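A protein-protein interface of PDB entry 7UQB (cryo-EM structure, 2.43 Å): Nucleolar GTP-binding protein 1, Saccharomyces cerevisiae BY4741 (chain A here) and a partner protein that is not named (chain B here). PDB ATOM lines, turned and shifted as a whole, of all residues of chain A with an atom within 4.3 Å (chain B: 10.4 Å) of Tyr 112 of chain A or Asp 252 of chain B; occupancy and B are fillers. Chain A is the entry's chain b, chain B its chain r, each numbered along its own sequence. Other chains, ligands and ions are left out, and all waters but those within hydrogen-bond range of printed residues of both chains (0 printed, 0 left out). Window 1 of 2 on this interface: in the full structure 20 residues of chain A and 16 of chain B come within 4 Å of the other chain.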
ATOM      1  N   VAL A 108     -10.327  21.582  -7.026  1.00  0.00           N
ATOM      2  CA  VAL A 108     -10.998  22.600  -7.834  1.00  0.00           C
ATOM      3  C   VAL A 108     -11.382  23.798  -6.976  1.00  0.00           C
ATOM      4  O   VAL A 108     -11.160  24.957  -7.362  1.00  0.00           O
ATOM      5  CB  VAL A 108     -12.230  21.995  -8.538  1.00  0.00           C
ATOM      6  CG1 VAL A 108     -13.139  23.093  -9.074  1.00  0.00           C
ATOM      7  CG2 VAL A 108     -11.803  21.067  -9.660  1.00  0.00           C
ATOM      8  N   ALA A 109     -11.952  23.538  -5.795  1.00  0.00           N
ATOM      9  CA  ALA A 109     -12.390  24.623  -4.922  1.00  0.00           C
ATOM     10  C   ALA A 109     -11.215  25.490  -4.485  1.00  0.00           C
ATOM     11  O   ALA A 109     -11.280  26.727  -4.557  1.00  0.00           O
ATOM     12  CB  ALA A 109     -13.121  24.056  -3.708  1.00  0.00           C
ATOM     13  N   ARG A 110     -10.121  24.856  -4.049  1.00  0.00           N
ATOM     14  CA  ARG A 110      -8.953  25.616  -3.609  1.00  0.00           C
ATOM     15  C   ARG A 110      -8.366  26.434  -4.754  1.00  0.00           C
ATOM     16  O   ARG A 110      -8.065  27.628  -4.592  1.00  0.00           O
ATOM     17  CB  ARG A 110      -7.900  24.675  -3.023  1.00  0.00           C
ATOM     18  CG  ARG A 110      -8.346  23.924  -1.778  1.00  0.00           C
ATOM     19  CD  ARG A 110      -7.174  23.218  -1.110  1.00  0.00           C
ATOM     20  NE  ARG A 110      -6.456  22.351  -2.036  1.00  0.00           N
ATOM     21  CZ  ARG A 110      -6.571  21.030  -2.074  1.00  0.00           C
ATOM     22  NH1 ARG A 110      -7.354  20.380  -1.229  1.00  0.00           N
ATOM     23  NH2 ARG A 110      -5.887  20.346  -2.986  1.00  0.00           N
ATOM     24  N   ASP A 111      -8.219  25.812  -5.930  1.00  0.00           N
ATOM     25  CA  ASP A 111      -7.613  26.495  -7.067  1.00  0.00           C
ATOM     26  C   ASP A 111      -8.432  27.703  -7.493  1.00  0.00           C
ATOM     27  O   ASP A 111      -7.879  28.777  -7.755  1.00  0.00           O
ATOM     28  CB  ASP A 111      -7.453  25.527  -8.238  1.00  0.00           C
ATOM     29  CG  ASP A 111      -6.375  24.493  -7.999  1.00  0.00           C
ATOM     30  OD1 ASP A 111      -5.739  24.530  -6.925  1.00  0.00           O
ATOM     31  OD2 ASP A 111      -6.165  23.638  -8.885  1.00  0.00           O
ATOM     32  N   TYR A 112      -9.756  27.564  -7.545  1.00  0.00           N
ATOM     33  CA  TYR A 112     -10.545  28.683  -8.034  1.00  0.00           C
ATOM     34  C   TYR A 112     -10.781  29.758  -6.984  1.00  0.00           C
ATOM     35  O   TYR A 112     -10.976  30.914  -7.357  1.00  0.00           O
ATOM     36  CB  TYR A 112     -11.863  28.185  -8.614  1.00  0.00           C
ATOM     37  CG  TYR A 112     -11.721  27.795 -10.067  1.00  0.00           C
ATOM     38  CD1 TYR A 112     -11.322  26.517 -10.428  1.00  0.00           C
ATOM     39  CD2 TYR A 112     -11.962  28.715 -11.077  1.00  0.00           C
ATOM     40  CE1 TYR A 112     -11.183  26.161 -11.754  1.00  0.00           C
ATOM     41  CE2 TYR A 112     -11.826  28.367 -12.406  1.00  0.00           C
ATOM     42  CZ  TYR A 112     -11.437  27.089 -12.738  1.00  0.00           C
ATOM     43  OH  TYR A 112     -11.295  26.736 -14.060  1.00  0.00           O
ATOM     44  N   VAL A 113     -10.720  29.437  -5.688  1.00  0.00           N
ATOM     45  CA  VAL A 113     -10.695  30.510  -4.695  1.00  0.00           C
ATOM     46  C   VAL A 113      -9.394  31.306  -4.808  1.00  0.00           C
ATOM     47  O   VAL A 113      -9.398  32.552  -4.778  1.00  0.00           O
ATOM     48  CB  VAL A 113     -10.912  29.935  -3.283  1.00  0.00           C
ATOM     49  CG1 VAL A 113     -10.536  30.952  -2.217  1.00  0.00           C
ATOM     50  CG2 VAL A 113     -12.362  29.516  -3.111  1.00  0.00           C
ATOM     51  N   ARG A 114      -8.268  30.605  -4.986  1.00  0.00           N
ATOM     52  CA  ARG A 114      -6.996  31.298  -5.168  1.00  0.00           C
ATOM     53  C   ARG A 114      -7.011  32.162  -6.424  1.00  0.00           C
ATOM     54  O   ARG A 114      -6.460  33.268  -6.430  1.00  0.00           O
ATOM     55  CB  ARG A 114      -5.846  30.292  -5.221  1.00  0.00           C
ATOM     56  CG  ARG A 114      -4.476  30.921  -5.023  1.00  0.00           C
ATOM     57  CD  ARG A 114      -3.344  29.915  -5.163  1.00  0.00           C
ATOM     58  NE  ARG A 114      -3.528  28.742  -4.320  1.00  0.00           N
ATOM     59  CZ  ARG A 114      -3.775  27.523  -4.779  1.00  0.00           C
ATOM     60  NH1 ARG A 114      -3.844  27.275  -6.076  1.00  0.00           N
ATOM     61  NH2 ARG A 114      -3.954  26.529  -3.916  1.00  0.00           N
ATOM     62  N   LEU A 115      -7.636  31.674  -7.499  1.00  0.00           N
ATOM     63  CA  LEU A 115      -7.767  32.480  -8.711  1.00  0.00           C
ATOM     64  C   LEU A 115      -8.683  33.680  -8.496  1.00  0.00           C
ATOM     65  O   LEU A 115      -8.383  34.785  -8.961  1.00  0.00           O
ATOM     66  CB  LEU A 115      -8.282  31.622  -9.863  1.00  0.00           C
ATOM     67  CG  LEU A 115      -7.267  30.710 -10.546  1.00  0.00           C
ATOM     68  CD1 LEU A 115      -7.934  29.918 -11.651  1.00  0.00           C
ATOM     69  CD2 LEU A 115      -6.108  31.526 -11.087  1.00  0.00           C
ATOM     70  N   LEU A 116      -9.804  33.484  -7.793  1.00  0.00           N
ATOM     71  CA  LEU A 116     -10.740  34.569  -7.526  1.00  0.00           C
ATOM     72  C   LEU A 116     -10.123  35.666  -6.680  1.00  0.00           C
ATOM     73  O   LEU A 116     -10.651  36.780  -6.658  1.00  0.00           O
ATOM     74  CB  LEU A 116     -11.991  34.035  -6.830  1.00  0.00           C
ATOM     75  CG  LEU A 116     -13.105  33.507  -7.731  1.00  0.00           C
ATOM     76  CD1 LEU A 116     -14.188  32.842  -6.904  1.00  0.00           C
ATOM     77  CD2 LEU A 116     -13.678  34.647  -8.549  1.00  0.00           C
ATOM     78  N   LEU A 128     -15.191  33.031 -13.396  1.00  0.00           N
ATOM     79  CA  LEU A 128     -14.377  32.097 -12.620  1.00  0.00           C
ATOM     80  C   LEU A 128     -15.236  31.200 -11.735  1.00  0.00           C
ATOM     81  O   LEU A 128     -14.994  29.987 -11.648  1.00  0.00           O
ATOM     82  CB  LEU A 128     -13.358  32.860 -11.774  1.00  0.00           C
ATOM     83  CG  LEU A 128     -12.224  33.563 -12.518  1.00  0.00           C
ATOM     84  CD1 LEU A 128     -11.324  34.302 -11.541  1.00  0.00           C
ATOM     85  CD2 LEU A 128     -11.427  32.573 -13.345  1.00  0.00           C
ATOM     86  N   ALA A 131     -16.941  28.674 -13.866  1.00  0.00           N
ATOM     87  CA  ALA A 131     -15.979  27.664 -14.292  1.00  0.00           C
ATOM     88  C   ALA A 131     -15.734  26.635 -13.197  1.00  0.00           C
ATOM     89  O   ALA A 131     -15.702  25.426 -13.466  1.00  0.00           O
ATOM     90  CB  ALA A 131     -14.668  28.328 -14.708  1.00  0.00           C
ATOM     91  N   ALA A 132     -15.567  27.098 -11.956  1.00  0.00           N
ATOM     92  CA  ALA A 132     -15.360  26.181 -10.839  1.00  0.00           C
ATOM     93  C   ALA A 132     -16.556  25.255 -10.654  1.00  0.00           C
ATOM     94  O   ALA A 132     -16.400  24.034 -10.507  1.00  0.00           O
ATOM     95  CB  ALA A 132     -15.096  26.969  -9.558  1.00  0.00           C
ATOM     96  N   ARG A 135     -16.801  22.679 -13.546  1.00  0.00           N
ATOM     97  CA  ARG A 135     -15.841  21.589 -13.390  1.00  0.00           C
ATOM     98  C   ARG A 135     -16.273  20.624 -12.292  1.00  0.00           C
ATOM     99  O   ARG A 135     -16.125  19.402 -12.440  1.00  0.00           O
ATOM    100  CB  ARG A 135     -14.448  22.147 -13.112  1.00  0.00           C
ATOM    101  CG  ARG A 135     -13.834  22.863 -14.302  1.00  0.00           C
ATOM    102  CD  ARG A 135     -12.552  23.571 -13.917  1.00  0.00           C
ATOM    103  NE  ARG A 135     -11.433  22.648 -13.787  1.00  0.00           N
ATOM    104  CZ  ARG A 135     -10.285  22.768 -14.440  1.00  0.00           C
ATOM    105  NH1 ARG A 135     -10.060  23.781 -15.261  1.00  0.00           N
ATOM    106  NH2 ARG A 135      -9.335  21.857 -14.256  1.00  0.00           N
ATOM    107  N   THR B 152      -2.311  41.283 -14.493  1.00  0.00           N
ATOM    108  CA  THR B 152      -3.560  40.668 -14.064  1.00  0.00           C
ATOM    109  C   THR B 152      -3.914  39.415 -14.851  1.00  0.00           C
ATOM    110  O   THR B 152      -4.860  38.716 -14.476  1.00  0.00           O
ATOM    111  CB  THR B 152      -4.710  41.671 -14.183  1.00  0.00           C
ATOM    112  OG1 THR B 152      -4.802  42.133 -15.536  1.00  0.00           O
ATOM    113  CG2 THR B 152      -4.478  42.856 -13.264  1.00  0.00           C
ATOM    114  N   LYS B 153      -3.190  39.120 -15.922  1.00  0.00           N
ATOM    115  CA  LYS B 153      -3.439  37.954 -16.754  1.00  0.00           C
ATOM    116  C   LYS B 153      -2.511  36.814 -16.350  1.00  0.00           C
ATOM    117  O   LYS B 153      -1.624  36.966 -15.509  1.00  0.00           O
ATOM    118  CB  LYS B 153      -3.251  38.304 -18.232  1.00  0.00           C
ATOM    119  CG  LYS B 153      -4.106  39.461 -18.714  1.00  0.00           C
ATOM    120  CD  LYS B 153      -5.573  39.085 -18.758  1.00  0.00           C
ATOM    121  CE  LYS B 153      -6.406  40.125 -19.494  1.00  0.00           C
ATOM    122  NZ  LYS B 153      -6.606  41.361 -18.700  1.00  0.00           N
ATOM    123  N   HIS B 154      -2.737  35.654 -16.956  1.00  0.00           N
ATOM    124  CA  HIS B 154      -1.882  34.500 -16.714  1.00  0.00           C
ATOM    125  C   HIS B 154      -0.586  34.632 -17.501  1.00  0.00           C
ATOM    126  O   HIS B 154      -0.567  35.166 -18.612  1.00  0.00           O
ATOM    127  CB  HIS B 154      -2.604  33.207 -17.092  1.00  0.00           C
ATOM    128  CG  HIS B 154      -3.720  32.845 -16.161  1.00  0.00           C
ATOM    129  ND1 HIS B 154      -3.765  31.645 -15.487  1.00  0.00           N
ATOM    130  CD2 HIS B 154      -4.825  33.529 -15.785  1.00  0.00           C
ATOM    131  CE1 HIS B 154      -4.853  31.603 -14.741  1.00  0.00           C
ATOM    132  NE2 HIS B 154      -5.514  32.735 -14.903  1.00  0.00           N
ATOM    133  N   ALA B 176       0.182  32.544  -8.352  1.00  0.00           N
ATOM    134  CA  ALA B 176      -1.076  31.838  -8.567  1.00  0.00           C
ATOM    135  C   ALA B 176      -1.534  31.920 -10.017  1.00  0.00           C
ATOM    136  O   ALA B 176      -2.270  31.043 -10.481  1.00  0.00           O
ATOM    137  CB  ALA B 176      -2.154  32.394  -7.640  1.00  0.00           C
ATOM    138  N   LEU B 177      -1.109  32.948 -10.746  1.00  0.00           N
ATOM    139  CA  LEU B 177      -1.493  33.121 -12.140  1.00  0.00           C
ATOM    140  C   LEU B 177      -0.495  32.511 -13.115  1.00  0.00           C
ATOM    141  O   LEU B 177      -0.712  32.595 -14.327  1.00  0.00           O
ATOM    142  CB  LEU B 177      -1.676  34.610 -12.454  1.00  0.00           C
ATOM    143  CG  LEU B 177      -2.784  35.335 -11.689  1.00  0.00           C
ATOM    144  CD1 LEU B 177      -2.883  36.790 -12.122  1.00  0.00           C
ATOM    145  CD2 LEU B 177      -4.110  34.628 -11.881  1.00  0.00           C
ATOM    146  N   GLN B 179       1.413  29.615 -15.257  1.00  0.00           N
ATOM    147  CA  GLN B 179       0.947  28.406 -15.917  1.00  0.00           C
ATOM    148  C   GLN B 179       2.130  27.598 -16.424  1.00  0.00           C
ATOM    149  O   GLN B 179       3.164  28.151 -16.807  1.00  0.00           O
ATOM    150  CB  GLN B 179       0.009  28.734 -17.088  1.00  0.00           C
ATOM    151  CG  GLN B 179      -1.338  29.294 -16.672  1.00  0.00           C
ATOM    152  CD  GLN B 179      -2.271  28.227 -16.131  1.00  0.00           C
ATOM    153  OE1 GLN B 179      -2.010  27.034 -16.261  1.00  0.00           O
ATOM    154  NE2 GLN B 179      -3.367  28.656 -15.523  1.00  0.00           N
ATOM    155  N   LYS B 181       1.154  24.175 -18.099  1.00  0.00           N
ATOM    156  CA  LYS B 181       0.591  23.195 -19.018  1.00  0.00           C
ATOM    157  C   LYS B 181      -0.676  23.763 -19.645  1.00  0.00           C
ATOM    158  O   LYS B 181      -1.309  24.672 -19.104  1.00  0.00           O
ATOM    159  CB  LYS B 181       0.278  21.866 -18.312  1.00  0.00           C
ATOM    160  CG  LYS B 181       1.478  21.171 -17.681  1.00  0.00           C
ATOM    161  CD  LYS B 181       1.082  19.860 -17.028  1.00  0.00           C
ATOM    162  CE  LYS B 181       0.753  18.804 -18.065  1.00  0.00           C
ATOM    163  NZ  LYS B 181       1.954  18.382 -18.824  1.00  0.00           N
ATOM    164  N   ALA B 182      -1.044  23.208 -20.799  1.00  0.00           N
ATOM    165  CA  ALA B 182      -2.223  23.643 -21.530  1.00  0.00           C
ATOM    166  C   ALA B 182      -2.921  22.439 -22.146  1.00  0.00           C
ATOM    167  O   ALA B 182      -2.284  21.437 -22.479  1.00  0.00           O
ATOM    168  CB  ALA B 182      -1.866  24.653 -22.628  1.00  0.00           C
ATOM    169  N   ASN B 183      -4.239  22.548 -22.299  1.00  0.00           N
ATOM    170  CA  ASN B 183      -5.015  21.538 -23.017  1.00  0.00           C
ATOM    171  C   ASN B 183      -4.871  21.823 -24.504  1.00  0.00           C
ATOM    172  O   ASN B 183      -5.476  22.758 -25.029  1.00  0.00           O
ATOM    173  CB  ASN B 183      -6.481  21.565 -22.597  1.00  0.00           C
ATOM    174  CG  ASN B 183      -6.667  21.506 -21.098  1.00  0.00           C
ATOM    175  OD1 ASN B 183      -6.461  20.466 -20.478  1.00  0.00           O
ATOM    176  ND2 ASN B 183      -7.067  22.623 -20.507  1.00  0.00           N
ATOM    177  N   LEU B 215      -0.090  35.163 -21.318  1.00  0.00           N
ATOM    178  CA  LEU B 215      -0.881  34.130 -21.977  1.00  0.00           C
ATOM    179  C   LEU B 215      -2.307  34.651 -22.109  1.00  0.00           C
ATOM    180  O   LEU B 215      -3.084  34.609 -21.150  1.00  0.00           O
ATOM    181  CB  LEU B 215      -0.837  32.821 -21.193  1.00  0.00           C
ATOM    182  CG  LEU B 215       0.520  32.136 -21.034  1.00  0.00           C
ATOM    183  CD1 LEU B 215       0.404  30.944 -20.101  1.00  0.00           C
ATOM    184  CD2 LEU B 215       1.057  31.710 -22.384  1.00  0.00           C
ATOM    185  N   THR B 216      -2.646  35.150 -23.292  1.00  0.00           N
ATOM    186  CA  THR B 216      -3.998  35.587 -23.607  1.00  0.00           C
ATOM    187  C   THR B 216      -4.458  34.881 -24.875  1.00  0.00           C
ATOM    188  O   THR B 216      -3.732  34.073 -25.459  1.00  0.00           O
ATOM    189  CB  THR B 216      -4.081  37.112 -23.772  1.00  0.00           C
ATOM    190  OG1 THR B 216      -3.021  37.566 -24.620  1.00  0.00           O
ATOM    191  CG2 THR B 216      -3.994  37.809 -22.422  1.00  0.00           C
ATOM    192  N   LYS B 217      -5.679  35.192 -25.297  1.00  0.00           N
ATOM    193  CA  LYS B 217      -6.241  34.584 -26.493  1.00  0.00           C
ATOM    194  C   LYS B 217      -5.459  35.011 -27.730  1.00  0.00           C
ATOM    195  O   LYS B 217      -5.133  36.187 -27.903  1.00  0.00           O
ATOM    196  CB  LYS B 217      -7.712  34.973 -26.633  1.00  0.00           C
ATOM    197  CG  LYS B 217      -8.477  34.161 -27.652  1.00  0.00           C
ATOM    198  CD  LYS B 217      -9.930  34.584 -27.702  1.00  0.00           C
ATOM    199  CE  LYS B 217     -10.685  33.817 -28.768  1.00  0.00           C
ATOM    200  NZ  LYS B 217     -12.081  34.301 -28.917  1.00  0.00           N
ATOM    201  N   VAL B 245      -3.342  29.847 -28.437  1.00  0.00           N
ATOM    202  CA  VAL B 245      -4.308  29.883 -27.347  1.00  0.00           C
ATOM    203  C   VAL B 245      -5.652  30.360 -27.880  1.00  0.00           C
ATOM    204  O   VAL B 245      -5.736  31.367 -28.593  1.00  0.00           O
ATOM    205  CB  VAL B 245      -3.795  30.782 -26.210  1.00  0.00           C
ATOM    206  CG1 VAL B 245      -4.825  30.893 -25.097  1.00  0.00           C
ATOM    207  CG2 VAL B 245      -2.482  30.244 -25.666  1.00  0.00           C
ATOM    208  N   THR B 246      -6.713  29.629 -27.543  1.00  0.00           N
ATOM    209  CA  THR B 246      -8.039  29.869 -28.091  1.00  0.00           C
ATOM    210  C   THR B 246      -9.049  30.338 -27.054  1.00  0.00           C
ATOM    211  O   THR B 246     -10.223  30.521 -27.394  1.00  0.00           O
ATOM    212  CB  THR B 246      -8.564  28.597 -28.768  1.00  0.00           C
ATOM    213  OG1 THR B 246      -8.493  27.502 -27.848  1.00  0.00           O
ATOM    214  CG2 THR B 246      -7.749  28.271 -30.004  1.00  0.00           C
ATOM    215  N   ASN B 247      -8.639  30.539 -25.808  1.00  0.00           N
ATOM    216  CA  ASN B 247      -9.550  30.927 -24.742  1.00  0.00           C
ATOM    217  C   ASN B 247      -8.970  32.116 -23.989  1.00  0.00           C
ATOM    218  O   ASN B 247      -7.899  32.629 -24.323  1.00  0.00           O
ATOM    219  CB  ASN B 247      -9.816  29.754 -23.790  1.00  0.00           C
ATOM    220  CG  ASN B 247      -8.606  29.394 -22.946  1.00  0.00           C
ATOM    221  OD1 ASN B 247      -7.465  29.500 -23.394  1.00  0.00           O
ATOM    222  ND2 ASN B 247      -8.853  28.966 -21.717  1.00  0.00           N
ATOM    223  N   GLU B 248      -9.687  32.555 -22.959  1.00  0.00           N
ATOM    224  CA  GLU B 248      -9.155  33.546 -22.032  1.00  0.00           C
ATOM    225  C   GLU B 248      -8.886  32.858 -20.701  1.00  0.00           C
ATOM    226  O   GLU B 248      -9.820  32.632 -19.911  1.00  0.00           O
ATOM    227  CB  GLU B 248     -10.121  34.723 -21.856  1.00  0.00           C
ATOM    228  CG  GLU B 248     -10.373  35.535 -23.131  1.00  0.00           C
ATOM    229  CD  GLU B 248      -9.247  36.510 -23.478  1.00  0.00           C
ATOM    230  OE1 GLU B 248      -8.140  36.412 -22.904  1.00  0.00           O
ATOM    231  OE2 GLU B 248      -9.477  37.389 -24.336  1.00  0.00           O
ATOM    232  N   PRO B 249      -7.635  32.477 -20.427  1.00  0.00           N
ATOM    233  CA  PRO B 249      -7.327  31.802 -19.157  1.00  0.00           C
ATOM    234  C   PRO B 249      -7.661  32.625 -17.930  1.00  0.00           C
ATOM    235  O   PRO B 249      -8.000  32.046 -16.894  1.00  0.00           O
ATOM    236  CB  PRO B 249      -5.821  31.516 -19.264  1.00  0.00           C
ATOM    237  CG  PRO B 249      -5.333  32.315 -20.436  1.00  0.00           C
ATOM    238  CD  PRO B 249      -6.491  32.465 -21.352  1.00  0.00           C
ATOM    239  N   ASP B 250      -7.593  33.954 -18.011  1.00  0.00           N
ATOM    240  CA  ASP B 250      -8.001  34.776 -16.879  1.00  0.00           C
ATOM    241  C   ASP B 250      -9.492  34.660 -16.591  1.00  0.00           C
ATOM    242  O   ASP B 250      -9.920  34.950 -15.469  1.00  0.00           O
ATOM    243  CB  ASP B 250      -7.629  36.238 -17.121  1.00  0.00           C
ATOM    244  CG  ASP B 250      -8.163  36.764 -18.437  1.00  0.00           C
ATOM    245  OD1 ASP B 250      -7.826  36.187 -19.492  1.00  0.00           O
ATOM    246  OD2 ASP B 250      -8.928  37.751 -18.414  1.00  0.00           O
ATOM    247  N   ARG B 251     -10.289  34.234 -17.570  1.00  0.00           N
ATOM    248  CA  ARG B 251     -11.720  34.033 -17.387  1.00  0.00           C
ATOM    249  C   ARG B 251     -12.090  32.604 -17.020  1.00  0.00           C
ATOM    250  O   ARG B 251     -13.012  32.402 -16.226  1.00  0.00           O
ATOM    251  CB  ARG B 251     -12.484  34.427 -18.654  1.00  0.00           C
ATOM    252  CG  ARG B 251     -12.489  35.908 -18.952  1.00  0.00           C
ATOM    253  CD  ARG B 251     -13.191  36.178 -20.264  1.00  0.00           C
ATOM    254  NE  ARG B 251     -12.935  37.527 -20.749  1.00  0.00           N
ATOM    255  CZ  ARG B 251     -13.317  37.980 -21.935  1.00  0.00           C
ATOM    256  NH1 ARG B 251     -13.989  37.218 -22.782  1.00  0.00           N
ATOM    257  NH2 ARG B 251     -13.007  39.225 -22.282  1.00  0.00           N
ATOM    258  N   ASP B 252     -11.421  31.595 -17.582  1.00  0.00           N
ATOM    259  CA  ASP B 252     -11.849  30.218 -17.346  1.00  0.00           C
ATOM    260  C   ASP B 252     -10.864  29.390 -16.525  1.00  0.00           C
ATOM    261  O   ASP B 252     -11.100  28.195 -16.329  1.00  0.00           O
ATOM    262  CB  ASP B 252     -12.151  29.510 -18.670  1.00  0.00           C
ATOM    263  CG  ASP B 252     -10.952  29.431 -19.576  1.00  0.00           C
ATOM    264  OD1 ASP B 252      -9.896  29.991 -19.217  1.00  0.00           O
ATOM    265  OD2 ASP B 252     -11.063  28.803 -20.650  1.00  0.00           O
ATOM    266  N   GLY B 253      -9.782  29.983 -16.030  1.00  0.00           N
ATOM    267  CA  GLY B 253      -8.884  29.295 -15.128  1.00  0.00           C
ATOM    268  C   GLY B 253      -7.925  28.314 -15.765  1.00  0.00           C
ATOM    269  O   GLY B 253      -7.160  27.668 -15.040  1.00  0.00           O
ATOM    270  N   CYS B 254      -7.927  28.183 -17.090  1.00  0.00           N
ATOM    271  CA  CYS B 254      -7.089  27.198 -17.756  1.00  0.00           C
ATOM    272  C   CYS B 254      -6.704  27.714 -19.133  1.00  0.00           C
ATOM    273  O   CYS B 254      -7.372  28.580 -19.701  1.00  0.00           O
ATOM    274  CB  CYS B 254      -7.803  25.848 -17.880  1.00  0.00           C
ATOM    275  SG  CYS B 254      -9.262  25.889 -18.947  1.00  0.00           S
ATOM    276  N   VAL B 255      -5.623  27.162 -19.673  1.00  0.00           N
ATOM    277  CA  VAL B 255      -5.160  27.500 -21.013  1.00  0.00           C
ATOM    278  C   VAL B 255      -5.595  26.393 -21.965  1.00  0.00           C
ATOM    279  O   VAL B 255      -5.256  25.221 -21.768  1.00  0.00           O
ATOM    280  CB  VAL B 255      -3.638  27.698 -21.056  1.00  0.00           C
ATOM    281  CG1 VAL B 255      -3.202  28.081 -22.461  1.00  0.00           C
ATOM    282  CG2 VAL B 255      -3.212  28.760 -20.057  1.00  0.00           C
ATOM    283  N   ASN B 256      -6.365  26.766 -22.982  1.00  0.00           N
ATOM    284  CA  ASN B 256      -6.760  25.874 -24.060  1.00  0.00           C
ATOM    285  C   ASN B 256      -6.113  26.356 -25.348  1.00  0.00           C
ATOM    286  O   ASN B 256      -6.097  27.557 -25.628  1.00  0.00           O
ATOM    287  CB  ASN B 256      -8.282  25.830 -24.218  1.00  0.00           C
ATOM    288  CG  ASN B 256      -8.977  25.250 -23.006  1.00  0.00           C
ATOM    289  OD1 ASN B 256      -8.554  24.234 -22.462  1.00  0.00           O
ATOM    290  ND2 ASN B 256     -10.049  25.896 -22.574  1.00  0.00           N
ATOM    291  N   ALA B 257      -5.581  25.426 -26.132  1.00  0.00           N
ATOM    292  CA  ALA B 257      -4.837  25.786 -27.327  1.00  0.00           C
ATOM    293  C   ALA B 257      -5.089  24.763 -28.423  1.00  0.00           C
ATOM    294  O   ALA B 257      -5.431  23.608 -28.164  1.00  0.00           O
ATOM    295  CB  ALA B 257      -3.334  25.894 -27.041  1.00  0.00           C
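Of the 13 printed residues of chain A, 5 touch a printed residue of chain B.
Printed residues of chain A that touch a printed residue of chain B: Tyr 112, Arg 114, Leu 115, Leu 128 and Ala 131.
Hydrophobic or aromatic side chains of chain B that line the printed part of chain A: His 154, Ala 176 and Leu 177.
Among the printed residues, no Asp or Glu carboxylate lies within 4 Å of a Lys or Arg side-chain nitrogen of the other chain.
A ring nitrogen (ND1) of His 154 of chain B sits close to the backbone carbonyl oxygen of Leu 177 of chain B (3.4 Å).
The side-chain carboxylate of Asp 252 of chain B lies within hydrogen-bond range of the side-chain amide nitrogen of Asn 247 of chain B.
The backbone NH (N) of Cys 254 of chain B lies close to the side-chain carboxylate (OD1) of Asp 252 of chain B (3.4 Å).
The side-chain carboxylate of Asp 252 of chain B sits close to the backbone carbonyl oxygen of Glu 248 of chain B (2.7 Å).
O of His 154 of chain B is in hydrogen-bond range of N of Leu 215 of chain B (2.7 Å).
NH1 of Arg 135 of chain A sits close to OH of Tyr 112 of chain A, at 3.4 Å.
The side-chain hydroxyl (OH) of Tyr 112 of chain A sits at hydrogen-bond distance from the backbone carbonyl oxygen (O) of Asp 252 of chain B.
Val 108 of chain A touches none of the printed residues of chain B.
No residue of chain B comes within 4 Å of Ala 109 of chain A.
No residue of chain B comes within 4 Å of Asp 111 of chain A.
Of chain B, only Asp 252 and Gly 253 come within 4 Å of Tyr 112 of chain A.
No residue of chain B comes within 4 Å of Val 113 of chain A.
Of the printed residues of chain B, Leu 115 of chain A touches His 154 (3.9 Å), Ala 176 (3.9 Å), Leu 177 (3.8 Å) and Gly 253 (3.7 Å).
Leu 128 of chain A touches just these residues of chain B: Asp 250 (3.5 Å) and Arg 251 (3.3 Å).
Of chain B, only Asp 252 comes within 4 Å of Ala 131 of chain A.
No residue of chain B comes within 4 Å of Ala 132 of chain A.
Of the printed residues of chain A, His 154 of chain B touches Leu 115 (3.9 Å).
Of the printed residues of chain A, Leu 177 of chain B touches Leu 115 (3.8 Å).
Printed residues of chain A within 4 Å of Asp 250 of chain B: Leu 128 (3.5 Å).
Of the printed residues of chain A, Arg 251 of chain B touches Leu 128 (3.3 Å).
Printed residues of chain A within 4 Å of Gly 253 of chain B: Tyr 112 (3.7 Å) and Leu 115 (3.7 Å).
Val 255 of chain B touches none of the printed residues of chain A.
Tyr 112 of chain A touches Gly 253 of chain B (OH to CA, 3.7 Å).
Arg 114 of chain A touches Ala 176 of chain B (CD to CB, 3.7 Å).
Leu 115 of chain A touches His 154 of chain B.
Ala 176 of chain B touches Leu 115 of chain A.
Leu 177 of chain B touches Leu 115 of chain A (CD2 to CD2, 3.8 Å).
Leu 115 of chain A touches Gly 253 of chain B.
Leu 128 of chain A touches Asp 250 of chain B.
CD2 of Leu 128 of chain A touches O of Arg 251 of chain B (3.3 Å).
Ala 131 of chain A touches Asp 252 of chain B (CB to O, 3.9 Å).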
